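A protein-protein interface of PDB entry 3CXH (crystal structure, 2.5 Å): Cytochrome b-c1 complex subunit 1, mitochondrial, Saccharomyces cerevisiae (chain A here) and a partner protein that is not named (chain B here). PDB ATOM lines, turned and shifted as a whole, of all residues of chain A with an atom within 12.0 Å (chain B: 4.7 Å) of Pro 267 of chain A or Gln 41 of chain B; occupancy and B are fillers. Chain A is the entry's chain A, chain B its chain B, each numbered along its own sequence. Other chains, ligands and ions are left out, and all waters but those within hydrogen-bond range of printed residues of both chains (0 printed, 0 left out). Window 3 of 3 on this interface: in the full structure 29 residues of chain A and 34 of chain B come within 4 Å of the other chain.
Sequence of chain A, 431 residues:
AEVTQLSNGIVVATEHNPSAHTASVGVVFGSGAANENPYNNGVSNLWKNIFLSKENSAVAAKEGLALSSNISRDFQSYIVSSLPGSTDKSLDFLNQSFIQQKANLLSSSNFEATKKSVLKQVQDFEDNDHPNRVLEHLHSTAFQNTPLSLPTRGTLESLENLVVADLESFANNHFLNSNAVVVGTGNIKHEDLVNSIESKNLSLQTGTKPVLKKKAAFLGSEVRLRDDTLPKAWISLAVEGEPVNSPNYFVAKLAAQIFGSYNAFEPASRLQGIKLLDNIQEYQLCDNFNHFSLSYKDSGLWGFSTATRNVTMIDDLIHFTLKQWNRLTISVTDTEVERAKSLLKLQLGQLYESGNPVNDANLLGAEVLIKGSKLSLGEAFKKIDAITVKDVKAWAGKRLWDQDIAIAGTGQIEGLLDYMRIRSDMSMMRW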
ATOM      1  N   SER A 261     -20.419  -9.238 -24.391  1.00  0.00           N
ATOM      2  CA  SER A 261     -20.012  -8.237 -25.362  1.00  0.00           C
ATOM      3  C   SER A 261     -21.121  -7.213 -25.448  1.00  0.00           C
ATOM      4  O   SER A 261     -22.266  -7.514 -25.126  1.00  0.00           O
ATOM      5  CB  SER A 261     -19.697  -8.862 -26.726  1.00  0.00           C
ATOM      6  OG  SER A 261     -20.816  -9.528 -27.268  1.00  0.00           O
ATOM      7  N   TYR A 262     -20.774  -6.016 -25.912  1.00  0.00           N
ATOM      8  CA  TYR A 262     -21.698  -4.899 -25.964  1.00  0.00           C
ATOM      9  C   TYR A 262     -21.431  -3.990 -27.151  1.00  0.00           C
ATOM     10  O   TYR A 262     -20.292  -3.837 -27.594  1.00  0.00           O
ATOM     11  CB  TYR A 262     -21.551  -4.123 -24.646  1.00  0.00           C
ATOM     12  CG  TYR A 262     -22.148  -2.737 -24.588  1.00  0.00           C
ATOM     13  CD1 TYR A 262     -21.332  -1.607 -24.643  1.00  0.00           C
ATOM     14  CD2 TYR A 262     -23.514  -2.550 -24.415  1.00  0.00           C
ATOM     15  CE1 TYR A 262     -21.864  -0.329 -24.523  1.00  0.00           C
ATOM     16  CE2 TYR A 262     -24.053  -1.273 -24.295  1.00  0.00           C
ATOM     17  CZ  TYR A 262     -23.220  -0.172 -24.350  1.00  0.00           C
ATOM     18  OH  TYR A 262     -23.748   1.087 -24.233  1.00  0.00           O
ATOM     19  N   ASN A 263     -22.500  -3.370 -27.636  1.00  0.00           N
ATOM     20  CA  ASN A 263     -22.445  -2.467 -28.769  1.00  0.00           C
ATOM     21  C   ASN A 263     -23.389  -1.320 -28.430  1.00  0.00           C
ATOM     22  O   ASN A 263     -24.602  -1.431 -28.575  1.00  0.00           O
ATOM     23  CB  ASN A 263     -22.917  -3.203 -30.019  1.00  0.00           C
ATOM     24  CG  ASN A 263     -22.821  -2.367 -31.279  1.00  0.00           C
ATOM     25  OD1 ASN A 263     -22.829  -2.914 -32.386  1.00  0.00           O
ATOM     26  ND2 ASN A 263     -22.747  -1.044 -31.130  1.00  0.00           N
ATOM     27  N   ALA A 264     -22.805  -0.220 -27.979  1.00  0.00           N
ATOM     28  CA  ALA A 264     -23.538   0.976 -27.575  1.00  0.00           C
ATOM     29  C   ALA A 264     -24.625   1.463 -28.508  1.00  0.00           C
ATOM     30  O   ALA A 264     -25.603   2.048 -28.052  1.00  0.00           O
ATOM     31  CB  ALA A 264     -22.563   2.113 -27.311  1.00  0.00           C
ATOM     32  N   PHE A 265     -24.455   1.238 -29.804  1.00  0.00           N
ATOM     33  CA  PHE A 265     -25.420   1.705 -30.793  1.00  0.00           C
ATOM     34  C   PHE A 265     -26.656   0.843 -31.046  1.00  0.00           C
ATOM     35  O   PHE A 265     -27.628   1.330 -31.620  1.00  0.00           O
ATOM     36  CB  PHE A 265     -24.701   1.983 -32.103  1.00  0.00           C
ATOM     37  CG  PHE A 265     -23.531   2.902 -31.958  1.00  0.00           C
ATOM     38  CD1 PHE A 265     -22.234   2.393 -31.923  1.00  0.00           C
ATOM     39  CD2 PHE A 265     -23.723   4.280 -31.842  1.00  0.00           C
ATOM     40  CE1 PHE A 265     -21.138   3.241 -31.775  1.00  0.00           C
ATOM     41  CE2 PHE A 265     -22.643   5.142 -31.693  1.00  0.00           C
ATOM     42  CZ  PHE A 265     -21.341   4.623 -31.659  1.00  0.00           C
ATOM     43  N   GLU A 266     -26.624  -0.414 -30.603  1.00  0.00           N
ATOM     44  CA  GLU A 266     -27.733  -1.356 -30.774  1.00  0.00           C
ATOM     45  C   GLU A 266     -28.612  -1.439 -29.520  1.00  0.00           C
ATOM     46  O   GLU A 266     -28.206  -1.998 -28.511  1.00  0.00           O
ATOM     47  CB  GLU A 266     -27.190  -2.753 -31.104  1.00  0.00           C
ATOM     48  CG  GLU A 266     -26.774  -2.969 -32.559  1.00  0.00           C
ATOM     49  CD  GLU A 266     -27.958  -3.095 -33.500  1.00  0.00           C
ATOM     50  OE1 GLU A 266     -27.864  -2.572 -34.639  1.00  0.00           O
ATOM     51  OE2 GLU A 266     -28.983  -3.716 -33.107  1.00  0.00           O
ATOM     52  N   PRO A 267     -29.869  -0.970 -29.611  1.00  0.00           N
ATOM     53  CA  PRO A 267     -30.848  -0.959 -28.517  1.00  0.00           C
ATOM     54  C   PRO A 267     -30.876  -2.186 -27.610  1.00  0.00           C
ATOM     55  O   PRO A 267     -30.760  -2.053 -26.394  1.00  0.00           O
ATOM     56  CB  PRO A 267     -32.168  -0.775 -29.257  1.00  0.00           C
ATOM     57  CG  PRO A 267     -31.771   0.136 -30.365  1.00  0.00           C
ATOM     58  CD  PRO A 267     -30.489  -0.490 -30.861  1.00  0.00           C
ATOM     59  N   ALA A 268     -31.029  -3.374 -28.190  1.00  0.00           N
ATOM     60  CA  ALA A 268     -31.083  -4.602 -27.395  1.00  0.00           C
ATOM     61  C   ALA A 268     -29.797  -4.875 -26.629  1.00  0.00           C
ATOM     62  O   ALA A 268     -29.834  -5.425 -25.533  1.00  0.00           O
ATOM     63  CB  ALA A 268     -31.430  -5.791 -28.265  1.00  0.00           C
ATOM     64  N   SER A 269     -28.663  -4.477 -27.194  1.00  0.00           N
ATOM     65  CA  SER A 269     -27.379  -4.689 -26.535  1.00  0.00           C
ATOM     66  C   SER A 269     -27.322  -3.883 -25.232  1.00  0.00           C
ATOM     67  O   SER A 269     -26.781  -4.346 -24.228  1.00  0.00           O
ATOM     68  CB  SER A 269     -26.226  -4.293 -27.476  1.00  0.00           C
ATOM     69  OG  SER A 269     -24.972  -4.790 -27.019  1.00  0.00           O
ATOM     70  N   ARG A 270     -27.924  -2.695 -25.252  1.00  0.00           N
ATOM     71  CA  ARG A 270     -27.955  -1.811 -24.087  1.00  0.00           C
ATOM     72  C   ARG A 270     -28.808  -2.352 -22.936  1.00  0.00           C
ATOM     73  O   ARG A 270     -28.643  -1.932 -21.789  1.00  0.00           O
ATOM     74  CB  ARG A 270     -28.457  -0.410 -24.477  1.00  0.00           C
ATOM     75  CG  ARG A 270     -27.609   0.325 -25.507  1.00  0.00           C
ATOM     76  CD  ARG A 270     -27.760   1.851 -25.395  1.00  0.00           C
ATOM     77  NE  ARG A 270     -29.114   2.303 -25.711  1.00  0.00           N
ATOM     78  CZ  ARG A 270     -29.528   2.710 -26.916  1.00  0.00           C
ATOM     79  NH1 ARG A 270     -30.794   3.096 -27.091  1.00  0.00           N
ATOM     80  NH2 ARG A 270     -28.685   2.752 -27.948  1.00  0.00           N
ATOM     81  N   LEU A 271     -29.677  -3.318 -23.230  1.00  0.00           N
ATOM     82  CA  LEU A 271     -30.567  -3.895 -22.225  1.00  0.00           C
ATOM     83  C   LEU A 271     -30.123  -5.204 -21.577  1.00  0.00           C
ATOM     84  O   LEU A 271     -30.816  -5.726 -20.696  1.00  0.00           O
ATOM     85  CB  LEU A 271     -31.949  -4.089 -22.833  1.00  0.00           C
ATOM     86  CG  LEU A 271     -32.534  -2.844 -23.496  1.00  0.00           C
ATOM     87  CD1 LEU A 271     -33.817  -3.198 -24.252  1.00  0.00           C
ATOM     88  CD2 LEU A 271     -32.783  -1.775 -22.439  1.00  0.00           C
ATOM     89  N   GLN A 272     -28.985  -5.742 -22.001  1.00  0.00           N
ATOM     90  CA  GLN A 272     -28.492  -7.011 -21.455  1.00  0.00           C
ATOM     91  C   GLN A 272     -28.354  -7.009 -19.942  1.00  0.00           C
ATOM     92  O   GLN A 272     -28.083  -5.976 -19.326  1.00  0.00           O
ATOM     93  CB  GLN A 272     -27.143  -7.388 -22.075  1.00  0.00           C
ATOM     94  CG  GLN A 272     -27.171  -7.629 -23.571  1.00  0.00           C
ATOM     95  CD  GLN A 272     -25.775  -7.717 -24.155  1.00  0.00           C
ATOM     96  OE1 GLN A 272     -25.216  -8.802 -24.296  1.00  0.00           O
ATOM     97  NE2 GLN A 272     -25.198  -6.567 -24.483  1.00  0.00           N
ATOM     98  N   GLY A 273     -28.550  -8.182 -19.352  1.00  0.00           N
ATOM     99  CA  GLY A 273     -28.440  -8.340 -17.915  1.00  0.00           C
ATOM    100  C   GLY A 273     -26.999  -8.452 -17.467  1.00  0.00           C
ATOM    101  O   GLY A 273     -26.586  -9.486 -16.913  1.00  0.00           O
ATOM    102  N   ILE A 274     -26.227  -7.398 -17.732  1.00  0.00           N
ATOM    103  CA  ILE A 274     -24.820  -7.337 -17.343  1.00  0.00           C
ATOM    104  C   ILE A 274     -24.645  -6.147 -16.400  1.00  0.00           C
ATOM    105  O   ILE A 274     -24.921  -5.002 -16.770  1.00  0.00           O
ATOM    106  CB  ILE A 274     -23.895  -7.176 -18.579  1.00  0.00           C
ATOM    107  CG1 ILE A 274     -24.174  -8.286 -19.599  1.00  0.00           C
ATOM    108  CG2 ILE A 274     -22.436  -7.232 -18.158  1.00  0.00           C
ATOM    109  CD1 ILE A 274     -23.363  -8.177 -20.890  1.00  0.00           C
ATOM    110  N   LEU A 277     -22.889  -2.860 -17.295  1.00  0.00           N
ATOM    111  CA  LEU A 277     -23.592  -1.898 -18.136  1.00  0.00           C
ATOM    112  C   LEU A 277     -24.201  -0.718 -17.381  1.00  0.00           C
ATOM    113  O   LEU A 277     -24.393   0.350 -17.955  1.00  0.00           O
ATOM    114  CB  LEU A 277     -24.632  -2.587 -19.008  1.00  0.00           C
ATOM    115  CG  LEU A 277     -24.074  -3.493 -20.110  1.00  0.00           C
ATOM    116  CD1 LEU A 277     -25.211  -3.937 -21.019  1.00  0.00           C
ATOM    117  CD2 LEU A 277     -23.013  -2.754 -20.915  1.00  0.00           C
ATOM    118  N   GLN A 281     -22.772   3.055 -19.095  1.00  0.00           N
ATOM    119  CA  GLN A 281     -23.708   3.768 -19.944  1.00  0.00           C
ATOM    120  C   GLN A 281     -24.027   5.228 -19.569  1.00  0.00           C
ATOM    121  O   GLN A 281     -24.318   6.041 -20.449  1.00  0.00           O
ATOM    122  CB  GLN A 281     -24.972   2.938 -20.145  1.00  0.00           C
ATOM    123  CG  GLN A 281     -24.681   1.655 -20.894  1.00  0.00           C
ATOM    124  CD  GLN A 281     -25.922   0.988 -21.451  1.00  0.00           C
ATOM    125  OE1 GLN A 281     -26.213   1.095 -22.636  1.00  0.00           O
ATOM    126  NE2 GLN A 281     -26.650   0.285 -20.600  1.00  0.00           N
ATOM    127  N   GLN A 284     -21.334   7.177 -21.024  1.00  0.00           N
ATOM    128  CA  GLN A 284     -20.998   6.464 -22.259  1.00  0.00           C
ATOM    129  C   GLN A 284     -19.498   6.293 -22.405  1.00  0.00           C
ATOM    130  O   GLN A 284     -18.840   6.959 -23.202  1.00  0.00           O
ATOM    131  CB  GLN A 284     -21.610   7.126 -23.492  1.00  0.00           C
ATOM    132  CG  GLN A 284     -21.733   6.146 -24.689  1.00  0.00           C
ATOM    133  CD  GLN A 284     -22.547   4.871 -24.359  1.00  0.00           C
ATOM    134  OE1 GLN A 284     -23.783   4.883 -24.380  1.00  0.00           O
ATOM    135  NE2 GLN A 284     -21.848   3.777 -24.051  1.00  0.00           N
ATOM    136  N   CYS A 286     -17.730   3.812 -23.609  1.00  0.00           N
ATOM    137  CA  CYS A 286     -17.178   3.174 -24.809  1.00  0.00           C
ATOM    138  C   CYS A 286     -18.243   2.895 -25.862  1.00  0.00           C
ATOM    139  O   CYS A 286     -19.433   2.897 -25.555  1.00  0.00           O
ATOM    140  CB  CYS A 286     -16.491   1.857 -24.447  1.00  0.00           C
ATOM    141  SG  CYS A 286     -17.647   0.543 -24.021  1.00  0.00           S
ATOM    142  N   ASP A 287     -17.806   2.687 -27.104  1.00  0.00           N
ATOM    143  CA  ASP A 287     -18.719   2.374 -28.199  1.00  0.00           C
ATOM    144  C   ASP A 287     -19.022   0.879 -28.217  1.00  0.00           C
ATOM    145  O   ASP A 287     -20.097   0.462 -28.644  1.00  0.00           O
ATOM    146  CB  ASP A 287     -18.132   2.809 -29.532  1.00  0.00           C
ATOM    147  CG  ASP A 287     -18.139   4.319 -29.708  1.00  0.00           C
ATOM    148  OD1 ASP A 287     -17.312   4.819 -30.495  1.00  0.00           O
ATOM    149  OD2 ASP A 287     -18.968   5.012 -29.068  1.00  0.00           O
ATOM    150  N   ASN A 288     -18.079   0.070 -27.742  1.00  0.00           N
ATOM    151  CA  ASN A 288     -18.282  -1.367 -27.692  1.00  0.00           C
ATOM    152  C   ASN A 288     -17.215  -2.087 -26.891  1.00  0.00           C
ATOM    153  O   ASN A 288     -16.142  -1.545 -26.618  1.00  0.00           O
ATOM    154  CB  ASN A 288     -18.335  -1.967 -29.104  1.00  0.00           C
ATOM    155  CG  ASN A 288     -17.047  -1.751 -29.880  1.00  0.00           C
ATOM    156  OD1 ASN A 288     -16.936  -0.802 -30.656  1.00  0.00           O
ATOM    157  ND2 ASN A 288     -16.058  -2.619 -29.659  1.00  0.00           N
ATOM    158  N   ARG A 339     -27.465 -17.221 -16.125  1.00  0.00           N
ATOM    159  CA  ARG A 339     -27.663 -16.482 -17.371  1.00  0.00           C
ATOM    160  C   ARG A 339     -26.527 -16.816 -18.328  1.00  0.00           C
ATOM    161  O   ARG A 339     -26.731 -16.914 -19.529  1.00  0.00           O
ATOM    162  CB  ARG A 339     -27.678 -14.969 -17.113  1.00  0.00           C
ATOM    163  CG  ARG A 339     -28.187 -14.152 -18.293  1.00  0.00           C
ATOM    164  CD  ARG A 339     -27.688 -12.710 -18.285  1.00  0.00           C
ATOM    165  NE  ARG A 339     -26.282 -12.641 -18.673  1.00  0.00           N
ATOM    166  CZ  ARG A 339     -25.818 -11.963 -19.719  1.00  0.00           C
ATOM    167  NH1 ARG A 339     -24.519 -11.984 -19.986  1.00  0.00           N
ATOM    168  NH2 ARG A 339     -26.644 -11.265 -20.491  1.00  0.00           N
ATOM    169  N   ARG B  37     -36.466  -1.105 -37.380  1.00  0.00           N
ATOM    170  CA  ARG B  37     -35.726  -0.631 -36.221  1.00  0.00           C
ATOM    171  C   ARG B  37     -36.640  -0.573 -34.985  1.00  0.00           C
ATOM    172  O   ARG B  37     -36.159  -0.588 -33.844  1.00  0.00           O
ATOM    173  CB  ARG B  37     -35.158   0.750 -36.545  1.00  0.00           C
ATOM    174  CG  ARG B  37     -33.724   0.989 -36.127  1.00  0.00           C
ATOM    175  CD  ARG B  37     -32.741   0.019 -36.763  1.00  0.00           C
ATOM    176  NE  ARG B  37     -32.223  -0.938 -35.785  1.00  0.00           N
ATOM    177  CZ  ARG B  37     -30.933  -1.156 -35.543  1.00  0.00           C
ATOM    178  NH1 ARG B  37     -30.573  -2.049 -34.640  1.00  0.00           N
ATOM    179  NH2 ARG B  37     -30.003  -0.492 -36.195  1.00  0.00           N
ATOM    180  N   PHE B  38     -37.952  -0.513 -35.216  1.00  0.00           N
ATOM    181  CA  PHE B  38     -38.926  -0.474 -34.122  1.00  0.00           C
ATOM    182  C   PHE B  38     -39.207  -1.875 -33.581  1.00  0.00           C
ATOM    183  O   PHE B  38     -39.655  -2.029 -32.435  1.00  0.00           O
ATOM    184  CB  PHE B  38     -40.245   0.169 -34.568  1.00  0.00           C
ATOM    185  CG  PHE B  38     -40.715   1.277 -33.668  1.00  0.00           C
ATOM    186  CD1 PHE B  38     -40.922   2.564 -34.173  1.00  0.00           C
ATOM    187  CD2 PHE B  38     -40.906   1.056 -32.305  1.00  0.00           C
ATOM    188  CE1 PHE B  38     -41.310   3.610 -33.331  1.00  0.00           C
ATOM    189  CE2 PHE B  38     -41.294   2.100 -31.458  1.00  0.00           C
ATOM    190  CZ  PHE B  38     -41.493   3.374 -31.976  1.00  0.00           C
ATOM    191  N   ASN B  39     -38.979  -2.896 -34.407  1.00  0.00           N
ATOM    192  CA  ASN B  39     -39.207  -4.269 -33.969  1.00  0.00           C
ATOM    193  C   ASN B  39     -38.389  -4.595 -32.733  1.00  0.00           C
ATOM    194  O   ASN B  39     -37.224  -4.200 -32.623  1.00  0.00           O
ATOM    195  CB  ASN B  39     -38.862  -5.272 -35.069  1.00  0.00           C
ATOM    196  CG  ASN B  39     -39.853  -5.260 -36.207  1.00  0.00           C
ATOM    197  OD1 ASN B  39     -39.555  -5.735 -37.300  1.00  0.00           O
ATOM    198  ND2 ASN B  39     -41.044  -4.724 -35.956  1.00  0.00           N
ATOM    199  N   PHE B  40     -39.016  -5.341 -31.827  1.00  0.00           N
ATOM    200  CA  PHE B  40     -38.430  -5.786 -30.563  1.00  0.00           C
ATOM    201  C   PHE B  40     -38.386  -4.735 -29.463  1.00  0.00           C
ATOM    202  O   PHE B  40     -37.833  -4.965 -28.380  1.00  0.00           O
ATOM    203  CB  PHE B  40     -37.083  -6.470 -30.784  1.00  0.00           C
ATOM    204  CG  PHE B  40     -37.191  -7.707 -31.618  1.00  0.00           C
ATOM    205  CD1 PHE B  40     -36.573  -7.782 -32.866  1.00  0.00           C
ATOM    206  CD2 PHE B  40     -37.986  -8.774 -31.193  1.00  0.00           C
ATOM    207  CE1 PHE B  40     -36.754  -8.895 -33.673  1.00  0.00           C
ATOM    208  CE2 PHE B  40     -38.168  -9.888 -31.997  1.00  0.00           C
ATOM    209  CZ  PHE B  40     -37.551  -9.949 -33.243  1.00  0.00           C
ATOM    210  N   GLN B  41     -38.987  -3.583 -29.748  1.00  0.00           N
ATOM    211  CA  GLN B  41     -39.112  -2.521 -28.768  1.00  0.00           C
ATOM    212  C   GLN B  41     -40.293  -2.973 -27.911  1.00  0.00           C
ATOM    213  O   GLN B  41     -40.751  -4.110 -28.035  1.00  0.00           O
ATOM    214  CB  GLN B  41     -39.434  -1.195 -29.447  1.00  0.00           C
ATOM    215  CG  GLN B  41     -38.243  -0.529 -30.108  1.00  0.00           C
ATOM    216  CD  GLN B  41     -37.184  -0.053 -29.116  1.00  0.00           C
ATOM    217  OE1 GLN B  41     -35.998  -0.024 -29.434  1.00  0.00           O
ATOM    218  NE2 GLN B  41     -37.613   0.344 -27.922  1.00  0.00           N
ATOM    219  N   ASN B  42     -40.809  -2.092 -27.068  1.00  0.00           N
ATOM    220  CA  ASN B  42     -41.924  -2.458 -26.211  1.00  0.00           C
ATOM    221  C   ASN B  42     -43.169  -2.911 -26.961  1.00  0.00           C
ATOM    222  O   ASN B  42     -43.494  -2.385 -28.036  1.00  0.00           O
ATOM    223  CB  ASN B  42     -42.337  -1.286 -25.318  1.00  0.00           C
ATOM    224  CG  ASN B  42     -41.337  -0.989 -24.224  1.00  0.00           C
ATOM    225  OD1 ASN B  42     -40.396  -1.746 -23.982  1.00  0.00           O
ATOM    226  ND2 ASN B  42     -41.543   0.129 -23.548  1.00  0.00           N
ATOM    227  N   THR B  43     -43.812  -3.941 -26.412  1.00  0.00           N
ATOM    228  CA  THR B  43     -45.087  -4.441 -26.922  1.00  0.00           C
ATOM    229  C   THR B  43     -46.019  -4.039 -25.779  1.00  0.00           C
ATOM    230  O   THR B  43     -45.554  -3.701 -24.687  1.00  0.00           O
ATOM    231  CB  THR B  43     -45.148  -5.974 -27.093  1.00  0.00           C
ATOM    232  OG1 THR B  43     -45.230  -6.607 -25.813  1.00  0.00           O
ATOM    233  CG2 THR B  43     -43.951  -6.487 -27.861  1.00  0.00           C
ATOM    234  N   ALA B  48     -39.210  -4.259 -23.879  1.00  0.00           N
ATOM    235  CA  ALA B  48     -37.979  -4.618 -24.564  1.00  0.00           C
ATOM    236  C   ALA B  48     -36.992  -5.168 -23.537  1.00  0.00           C
ATOM    237  O   ALA B  48     -36.328  -6.178 -23.783  1.00  0.00           O
ATOM    238  CB  ALA B  48     -37.399  -3.400 -25.265  1.00  0.00           C
ATOM    239  N   GLU B 102     -39.896   6.004 -27.444  1.00  0.00           N
ATOM    240  CA  GLU B 102     -39.070   4.947 -28.004  1.00  0.00           C
ATOM    241  C   GLU B 102     -38.560   5.395 -29.375  1.00  0.00           C
ATOM    242  O   GLU B 102     -37.424   5.105 -29.752  1.00  0.00           O
ATOM    243  CB  GLU B 102     -39.872   3.660 -28.134  1.00  0.00           C
ATOM    244  CG  GLU B 102     -40.509   3.228 -26.840  1.00  0.00           C
ATOM    245  CD  GLU B 102     -41.079   1.834 -26.920  1.00  0.00           C
ATOM    246  OE1 GLU B 102     -42.295   1.703 -27.191  1.00  0.00           O
ATOM    247  OE2 GLU B 102     -40.304   0.870 -26.713  1.00  0.00           O
ATOM    248  N   SER B 106     -34.693   5.470 -28.876  1.00  0.00           N
ATOM    249  CA  SER B 106     -34.020   4.270 -29.385  1.00  0.00           C
ATOM    250  C   SER B 106     -33.993   4.085 -30.898  1.00  0.00           C
ATOM    251  O   SER B 106     -32.935   3.847 -31.482  1.00  0.00           O
ATOM    252  CB  SER B 106     -34.630   3.010 -28.762  1.00  0.00           C
ATOM    253  OG  SER B 106     -34.507   3.025 -27.354  1.00  0.00           O
ATOM    254  N   VAL B 107     -35.170   4.176 -31.512  1.00  0.00           N
ATOM    255  CA  VAL B 107     -35.344   3.986 -32.944  1.00  0.00           C
ATOM    256  C   VAL B 107     -34.632   4.993 -33.843  1.00  0.00           C
ATOM    257  O   VAL B 107     -33.826   4.600 -34.686  1.00  0.00           O
ATOM    258  CB  VAL B 107     -36.849   3.906 -33.297  1.00  0.00           C
ATOM    259  CG1 VAL B 107     -37.040   3.623 -34.779  1.00  0.00           C
ATOM    260  CG2 VAL B 107     -37.520   2.830 -32.454  1.00  0.00           C
ATOM    261  N   ALA B 110     -30.822   4.603 -33.663  1.00  0.00           N
ATOM    262  CA  ALA B 110     -30.362   3.358 -34.289  1.00  0.00           C
ATOM    263  C   ALA B 110     -30.352   3.501 -35.815  1.00  0.00           C
ATOM    264  O   ALA B 110     -29.396   3.098 -36.479  1.00  0.00           O
ATOM    265  CB  ALA B 110     -31.236   2.190 -33.863  1.00  0.00           C
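Hydrophobic or aromatic side chains of chain B within 4 Å of the printed part of chain A: Ala 48.
Hydrophobic or aromatic side chains of chain A within 4 Å of the printed part of chain B: Pro 267 and Leu 271.
Along chain A the printed residues that touch a printed residue of chain B span positions 266 to 271.
Among the printed residues, 4 pairs touch across the chains.
Among the printed residues, Asp or Glu carboxylates within 4 Å of a Lys or Arg side-chain nitrogen of the other chain: Glu 266 of chain A with Arg 37 of chain B (2.8 Å).
Tyr 262 of chain A touches none of the printed residues of chain B.
Printed residues of chain B within 4 Å of Glu 266 of chain A: Arg 37.
Pro 267 of chain A touches just one residue of chain B: Gln 41 (3.9 Å).
Printed residues of chain B within 4 Å of Arg 270 of chain A: Ser 106 (3.7 Å).
Printed residues of chain B within 4 Å of Leu 271 of chain A: Ala 48 (3.7 Å).
Of chain A, only Glu 266 (2.8 Å) comes within 4 Å of Arg 37 of chain B.
No residue of chain A comes within 4 Å of Asn 39 of chain B.
Of the printed residues of chain A, Gln 41 of chain B touches Pro 267 (3.9 Å).
Asn 42 of chain B touches none of the printed residues of chain A.
No residue of chain A comes within 4 Å of Thr 43 of chain B.
No residue of chain A comes within 4 Å of Glu 102 of chain B.
Of chain A, only Arg 270 comes within 4 Å of Ser 106 of chain B.
No residue of chain A comes within 4 Å of Ala 110 of chain B.
The nearest residue of chain B that does not touch Pro 267 of chain A is Ser 106 of chain B (4.05 Å).
OE1 of Glu 266 of chain A lies within salt-bridge range of NH1 of Arg 37 of chain B (2.8 Å).
Among the printed residues, pairs that only touch across the chains: Arg 270 of chain A with Ser 106 of chain B (3.7 Å), Leu 271 of chain A with Ala 48 of chain B (3.7 Å) and Pro 267 of chain A with Gln 41 of chain B (3.9 Å).
The backbone carbonyl oxygen of Ala 264 of chain A lies within hydrogen-bond range of the guanidinium group of Arg 270 of chain A.
The side-chain amide nitrogen (NE2) of Gln 281 of chain A lies within hydrogen-bond range of the backbone carbonyl oxygen (O) of Arg 270 of chain A.
OE2 of Glu 102 of chain B lies within hydrogen-bond range of NE2 of Gln 41 of chain B (3.0 Å).
N of Ala 48 of chain B sits at hydrogen-bond distance from OD1 of Asn 42 of chain B (2.8 Å).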
